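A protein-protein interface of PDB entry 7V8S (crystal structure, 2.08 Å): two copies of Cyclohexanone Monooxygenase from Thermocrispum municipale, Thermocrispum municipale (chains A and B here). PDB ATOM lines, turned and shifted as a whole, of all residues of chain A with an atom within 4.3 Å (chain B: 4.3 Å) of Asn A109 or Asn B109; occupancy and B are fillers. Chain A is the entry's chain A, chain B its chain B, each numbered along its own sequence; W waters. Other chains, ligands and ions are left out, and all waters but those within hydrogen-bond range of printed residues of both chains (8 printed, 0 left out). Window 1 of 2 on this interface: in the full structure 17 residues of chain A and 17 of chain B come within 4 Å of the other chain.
The backbone NH of Asn A109 lies within hydrogen-bond range of the backbone carbonyl oxygen of Glu A39 (2.8 Å). The backbone carbonyl oxygen of Glu A39 sits at hydrogen-bond distance from the backbone NH of Thr A110, 2.9 Å away. The backbone NH (N) of Asn A109 lies within hydrogen-bond range of the backbone carbonyl oxygen (O) of Gly A41 (2.9 Å). The backbone carbonyl oxygen (O) of Gln B107 lies within hydrogen-bond range of the backbone NH (N) of Glu B39, at 3.1 Å. O of Glu B39 lies within hydrogen-bond range of N of Asn B109, 2.9 Å away. The backbone carbonyl oxygen of Gly B41 sits at hydrogen-bond distance from the backbone NH of Asn B109, at 2.9 Å.
Of the printed residues of chain B, Gly A42 touches Gly B130. Of chain B, only Gln B107, Asn B109, Thr B110 and Gly B130 come within 4 Å of Asn A109. Glu B39 touches none of the printed residues of chain A. Printed residues of chain A within 4 Å of Lys B40: Gly A130. Of the printed residues of chain A, Asn B109 touches Gln A107, Asn A109, Thr A110 and Gly A130. Printed residues of chain A within 4 Å of Thr B110: Asn A109. Of the printed residues of chain A, Gly B130 touches Lys A40 (3.4 Å), Gly A41 (3.6 Å), Gly A42 (2.7 Å) and Asn A109 (3.6 Å). The nearest residue of chain B that does not touch Asn A109 is Leu B108 (4.1 Å).
Printed residues of chain A that touch a printed residue of chain B: Lys A40, Gly A41, Gly A42, Gln A107, Asn A109, Thr A110 and Gly A130. Among the printed residues, 13 pairs touch across the chains.
Water W6 lies within hydrogen-bond range of O of Asn B109, N of Glu B111 and O of Asn A109. Water W1 bridges the backbone carbonyl oxygen (O) of Leu A108 and the side-chain amide oxygen (OD1) of Asn B109. Water W2 bridges O of Leu B108 (2.7 Å) and OD1 of Asn A109 (3.1 Å). Water W8 lies within hydrogen-bond range of O of Asn A109 (2.7 Å), N of Glu A111 (3.3 Å) and O of Asn B109 (3.4 Å). Water W7 lies within hydrogen-bond range of O of Gly B42, OD1 of Asn B109 and NE2 of Gln A107. Water W5 bridges the side-chain amide nitrogen of Asn A109 (2.7 Å) and the backbone NH of Gly B130 (2.8 Å).
Among the printed residues, pairs that only touch across the chains: Thr A110 with Asn B109 (3.3 Å), Gly A130 with Lys B40 (3.4 Å), Lys A40 with Gly B130 (3.4 Å), Gly A130 with Gly B41 (3.5 Å), Gly A41 with Gly B130 (3.6 Å), Gly A130 with Asn B109 (3.6 Å) and Asn A109 with Gly B130 (3.6 Å).
Lys A40 touches Gly B130, and with the chains exchanged Gly A130 touches Lys B40. Gly A41 touches Gly B130, and with the chains exchanged Gly A130 touches Gly B41. Gly A42 touches Gly B130, and with the chains exchanged Gly A130 touches Gly B42. Asn A109 touches Gly B130, and with the chains exchanged Gly A130 touches Asn B109. Positions printed for both chains: 39, 40, 41, 42, 107, 108, 109, 110, 111 and 130. Of the 13 pairs that touch across the chains among the printed residues, 13 have their exchanged pair printed and touching as well.
The backbone NH of Gly A42 lies within hydrogen-bond range of the backbone carbonyl oxygen of Gly B130, at 2.7 Å. NE2 of Gln A107 lies within hydrogen-bond range of OD1 of Asn B109, at 3.5 Å. OD1 of Asn A109 sits at hydrogen-bond distance from NE2 of Gln B107. The backbone carbonyl oxygen (O) of Asn A109 lies close to the backbone carbonyl oxygen (O) of Asn B109 (2.6 Å). OD1 of Asn A109 sits close to OG1 of Thr B110 (3.4 Å). The backbone NH (N) of Gly B42 sits at hydrogen-bond distance from the backbone carbonyl oxygen (O) of Gly A130, 2.8 Å away.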
ATOM      1  N   GLU A  39     -25.949  15.578  18.521  1.00  0.00           N
ATOM      2  CA  GLU A  39     -25.206  15.508  17.239  1.00  0.00           C
ATOM      3  C   GLU A  39     -25.504  16.796  16.468  1.00  0.00           C
ATOM      4  O   GLU A  39     -26.704  17.083  16.236  1.00  0.00           O
ATOM      5  CB  GLU A  39     -25.632  14.272  16.454  1.00  0.00           C
ATOM      6  CG  GLU A  39     -25.226  14.290  14.986  1.00  0.00           C
ATOM      7  CD  GLU A  39     -23.724  14.327  14.738  1.00  0.00           C
ATOM      8  OE1 GLU A  39     -23.028  13.469  15.287  1.00  0.00           O
ATOM      9  OE2 GLU A  39     -23.263  15.204  13.982  1.00  0.00           O
ATOM     10  N   LYS A  40     -24.462  17.538  16.093  1.00  0.00           N
ATOM     11  CA  LYS A  40     -24.598  18.861  15.426  1.00  0.00           C
ATOM     12  C   LYS A  40     -25.078  18.644  13.980  1.00  0.00           C
ATOM     13  O   LYS A  40     -25.670  19.580  13.414  1.00  0.00           O
ATOM     14  CB  LYS A  40     -23.283  19.648  15.512  1.00  0.00           C
ATOM     15  CG  LYS A  40     -22.101  19.016  14.792  1.00  0.00           C
ATOM     16  CD  LYS A  40     -20.892  19.912  14.735  1.00  0.00           C
ATOM     17  CE  LYS A  40     -19.663  19.164  14.252  1.00  0.00           C
ATOM     18  NZ  LYS A  40     -18.447  19.964  14.507  1.00  0.00           N
ATOM     19  N   GLY A  41     -24.820  17.459  13.415  1.00  0.00           N
ATOM     20  CA  GLY A  41     -25.266  17.061  12.069  1.00  0.00           C
ATOM     21  C   GLY A  41     -26.777  16.968  11.977  1.00  0.00           C
ATOM     22  O   GLY A  41     -27.406  16.740  13.024  1.00  0.00           O
ATOM     23  N   GLY A  42     -27.330  17.120  10.764  1.00  0.00           N
ATOM     24  CA  GLY A  42     -28.782  17.081  10.492  1.00  0.00           C
ATOM     25  C   GLY A  42     -29.322  15.663  10.420  1.00  0.00           C
ATOM     26  O   GLY A  42     -30.555  15.505  10.315  1.00  0.00           O
ATOM     27  N   GLN A 107     -30.790  13.957  19.676  1.00  0.00           N
ATOM     28  CA  GLN A 107     -31.224  15.325  19.298  1.00  0.00           C
ATOM     29  C   GLN A 107     -30.247  15.842  18.235  1.00  0.00           C
ATOM     30  O   GLN A 107     -29.067  16.121  18.567  1.00  0.00           O
ATOM     31  CB  GLN A 107     -31.304  16.218  20.534  1.00  0.00           C
ATOM     32  CG  GLN A 107     -31.979  17.555  20.276  1.00  0.00           C
ATOM     33  CD  GLN A 107     -31.975  18.375  21.543  1.00  0.00           C
ATOM     34  OE1 GLN A 107     -32.455  17.938  22.583  1.00  0.00           O
ATOM     35  NE2 GLN A 107     -31.402  19.563  21.484  1.00  0.00           N
ATOM     36  N   LEU A 108     -30.733  15.928  16.996  1.00  0.00           N
ATOM     37  CA  LEU A 108     -29.950  16.343  15.814  1.00  0.00           C
ATOM     38  C   LEU A 108     -29.814  17.869  15.800  1.00  0.00           C
ATOM     39  O   LEU A 108     -30.516  18.552  16.602  1.00  0.00           O
ATOM     40  CB  LEU A 108     -30.644  15.803  14.564  1.00  0.00           C
ATOM     41  CG  LEU A 108     -30.687  14.279  14.477  1.00  0.00           C
ATOM     42  CD1 LEU A 108     -31.594  13.824  13.338  1.00  0.00           C
ATOM     43  CD2 LEU A 108     -29.281  13.717  14.318  1.00  0.00           C
ATOM     44  N   ASN A 109     -28.869  18.360  14.995  1.00  0.00           N
ATOM     45  CA  ASN A 109     -28.635  19.803  14.716  1.00  0.00           C
ATOM     46  C   ASN A 109     -28.070  20.493  15.961  1.00  0.00           C
ATOM     47  O   ASN A 109     -27.969  21.722  15.951  1.00  0.00           O
ATOM     48  CB  ASN A 109     -29.913  20.466  14.189  1.00  0.00           C
ATOM     49  CG  ASN A 109     -30.258  19.982  12.797  1.00  0.00           C
ATOM     50  OD1 ASN A 109     -31.284  19.342  12.578  1.00  0.00           O
ATOM     51  ND2 ASN A 109     -29.381  20.254  11.854  1.00  0.00           N
ATOM     52  N   THR A 110     -27.710  19.732  16.993  1.00  0.00           N
ATOM     53  CA  THR A 110     -27.370  20.276  18.330  1.00  0.00           C
ATOM     54  C   THR A 110     -25.865  20.115  18.562  1.00  0.00           C
ATOM     55  O   THR A 110     -25.413  18.974  18.804  1.00  0.00           O
ATOM     56  CB  THR A 110     -28.238  19.623  19.411  1.00  0.00           C
ATOM     57  OG1 THR A 110     -29.614  19.824  19.064  1.00  0.00           O
ATOM     58  CG2 THR A 110     -27.965  20.200  20.783  1.00  0.00           C
ATOM     59  N   GLU A 111     -25.130  21.222  18.441  1.00  0.00           N
ATOM     60  CA  GLU A 111     -23.686  21.318  18.754  1.00  0.00           C
ATOM     61  C   GLU A 111     -23.540  21.649  20.241  1.00  0.00           C
ATOM     62  O   GLU A 111     -24.118  22.672  20.699  1.00  0.00           O
ATOM     63  CB  GLU A 111     -23.010  22.390  17.903  1.00  0.00           C
ATOM     64  CG  GLU A 111     -21.513  22.499  18.134  1.00  0.00           C
ATOM     65  CD  GLU A 111     -20.840  23.529  17.247  1.00  0.00           C
ATOM     66  OE1 GLU A 111     -21.554  24.343  16.643  1.00  0.00           O
ATOM     67  OE2 GLU A 111     -19.616  23.512  17.159  1.00  0.00           O
ATOM     68  N   GLY A 130     -27.890  25.965  20.619  1.00  0.00           N
ATOM     69  CA  GLY A 130     -29.325  26.311  20.707  1.00  0.00           C
ATOM     70  C   GLY A 130     -29.748  26.906  22.048  1.00  0.00           C
ATOM     71  O   GLY A 130     -30.935  27.269  22.176  1.00  0.00           O
ATOM     72  N   GLU B  39     -34.983  27.546  12.972  1.00  0.00           N
ATOM     73  CA  GLU B  39     -34.670  28.374  14.166  1.00  0.00           C
ATOM     74  C   GLU B  39     -33.412  27.783  14.818  1.00  0.00           C
ATOM     75  O   GLU B  39     -33.430  26.592  15.127  1.00  0.00           O
ATOM     76  CB  GLU B  39     -35.894  28.406  15.093  1.00  0.00           C
ATOM     77  CG  GLU B  39     -35.638  28.978  16.489  1.00  0.00           C
ATOM     78  CD  GLU B  39     -35.071  30.389  16.527  1.00  0.00           C
ATOM     79  OE1 GLU B  39     -35.761  31.320  16.049  1.00  0.00           O
ATOM     80  OE2 GLU B  39     -33.940  30.557  17.023  1.00  0.00           O
ATOM     81  N   LYS B  40     -32.361  28.582  15.017  1.00  0.00           N
ATOM     82  CA  LYS B  40     -31.081  28.067  15.570  1.00  0.00           C
ATOM     83  C   LYS B  40     -31.225  27.781  17.074  1.00  0.00           C
ATOM     84  O   LYS B  40     -30.435  26.976  17.568  1.00  0.00           O
ATOM     85  CB  LYS B  40     -29.911  29.009  15.275  1.00  0.00           C
ATOM     86  CG  LYS B  40     -30.035  30.433  15.802  1.00  0.00           C
ATOM     87  CD  LYS B  40     -28.759  31.206  15.591  1.00  0.00           C
ATOM     88  CE  LYS B  40     -28.919  32.690  15.807  1.00  0.00           C
ATOM     89  NZ  LYS B  40     -27.689  33.424  15.421  1.00  0.00           N
ATOM     90  N   GLY B  41     -32.198  28.395  17.759  1.00  0.00           N
ATOM     91  CA  GLY B  41     -32.492  28.123  19.182  1.00  0.00           C
ATOM     92  C   GLY B  41     -33.116  26.748  19.402  1.00  0.00           C
ATOM     93  O   GLY B  41     -33.699  26.186  18.429  1.00  0.00           O
ATOM     94  N   GLY B  42     -33.018  26.233  20.637  1.00  0.00           N
ATOM     95  CA  GLY B  42     -33.574  24.929  21.058  1.00  0.00           C
ATOM     96  C   GLY B  42     -35.067  24.978  21.365  1.00  0.00           C
ATOM     97  O   GLY B  42     -35.624  23.926  21.653  1.00  0.00           O
ATOM     98  N   GLN B 107     -38.172  23.508  12.517  1.00  0.00           N
ATOM     99  CA  GLN B 107     -36.969  22.696  12.830  1.00  0.00           C
ATOM    100  C   GLN B 107     -36.069  23.499  13.774  1.00  0.00           C
ATOM    101  O   GLN B 107     -35.476  24.499  13.331  1.00  0.00           O
ATOM    102  CB  GLN B 107     -36.263  22.304  11.531  1.00  0.00           C
ATOM    103  CG  GLN B 107     -35.073  21.383  11.756  1.00  0.00           C
ATOM    104  CD  GLN B 107     -34.576  20.812  10.451  1.00  0.00           C
ATOM    105  OE1 GLN B 107     -35.348  20.282   9.659  1.00  0.00           O
ATOM    106  NE2 GLN B 107     -33.279  20.920  10.218  1.00  0.00           N
ATOM    107  N   LEU B 108     -35.968  23.075  15.030  1.00  0.00           N
ATOM    108  CA  LEU B 108     -35.160  23.774  16.061  1.00  0.00           C
ATOM    109  C   LEU B 108     -33.681  23.381  15.931  1.00  0.00           C
ATOM    110  O   LEU B 108     -33.359  22.432  15.171  1.00  0.00           O
ATOM    111  CB  LEU B 108     -35.730  23.448  17.445  1.00  0.00           C
ATOM    112  CG  LEU B 108     -37.173  23.903  17.653  1.00  0.00           C
ATOM    113  CD1 LEU B 108     -37.801  23.255  18.875  1.00  0.00           C
ATOM    114  CD2 LEU B 108     -37.244  25.415  17.742  1.00  0.00           C
ATOM    115  N   ASN B 109     -32.816  24.141  16.610  1.00  0.00           N
ATOM    116  CA  ASN B 109     -31.345  23.934  16.714  1.00  0.00           C
ATOM    117  C   ASN B 109     -30.690  24.087  15.340  1.00  0.00           C
ATOM    118  O   ASN B 109     -29.508  23.722  15.214  1.00  0.00           O
ATOM    119  CB  ASN B 109     -31.029  22.587  17.368  1.00  0.00           C
ATOM    120  CG  ASN B 109     -31.563  22.518  18.782  1.00  0.00           C
ATOM    121  OD1 ASN B 109     -32.525  21.799  19.064  1.00  0.00           O
ATOM    122  ND2 ASN B 109     -30.968  23.296  19.665  1.00  0.00           N
ATOM    123  N   THR B 110     -31.396  24.667  14.368  1.00  0.00           N
ATOM    124  CA  THR B 110     -30.975  24.674  12.947  1.00  0.00           C
ATOM    125  C   THR B 110     -30.656  26.110  12.518  1.00  0.00           C
ATOM    126  O   THR B 110     -31.597  26.907  12.258  1.00  0.00           O
ATOM    127  CB  THR B 110     -31.994  23.950  12.062  1.00  0.00           C
ATOM    128  OG1 THR B 110     -32.130  22.622  12.566  1.00  0.00           O
ATOM    129  CG2 THR B 110     -31.568  23.903  10.612  1.00  0.00           C
ATOM    130  N   GLU B 111     -29.360  26.417  12.475  1.00  0.00           N
ATOM    131  CA  GLU B 111     -28.824  27.694  11.958  1.00  0.00           C
ATOM    132  C   GLU B 111     -28.709  27.596  10.439  1.00  0.00           C
ATOM    133  O   GLU B 111     -28.103  26.611   9.942  1.00  0.00           O
ATOM    134  CB  GLU B 111     -27.463  28.011  12.569  1.00  0.00           C
ATOM    135  CG  GLU B 111     -27.049  29.441  12.305  1.00  0.00           C
ATOM    136  CD  GLU B 111     -25.675  29.818  12.822  1.00  0.00           C
ATOM    137  OE1 GLU B 111     -24.946  28.920  13.270  1.00  0.00           O
ATOM    138  OE2 GLU B 111     -25.348  31.013  12.762  1.00  0.00           O
ATOM    139  N   GLY B 130     -26.080  22.060  10.109  1.00  0.00           N
ATOM    140  CA  GLY B 130     -26.193  20.588  10.205  1.00  0.00           C
ATOM    141  C   GLY B 130     -25.926  19.859   8.893  1.00  0.00           C
ATOM    142  O   GLY B 130     -26.025  18.616   8.904  1.00  0.00           O
HETATM  143  O   HOH W   1     -32.991  19.181  17.299  1.00  0.00           O
HETATM  144  O   HOH W   2     -33.501  19.796  14.673  1.00  0.00           O
HETATM  145  O   HOH W   3     -28.270  23.302  19.698  1.00  0.00           O
HETATM  146  O   HOH W   4     -32.152  17.878  10.389  1.00  0.00           O
HETATM  147  O   HOH W   5     -28.350  22.772  11.519  1.00  0.00           O
HETATM  148  O   HOH W   6     -27.445  24.175  13.754  1.00  0.00           O
HETATM  149  O   HOH W   7     -34.032  21.742  21.578  1.00  0.00           O
HETATM  150  O   HOH W   8     -26.816  23.780  17.254  1.00  0.00           O
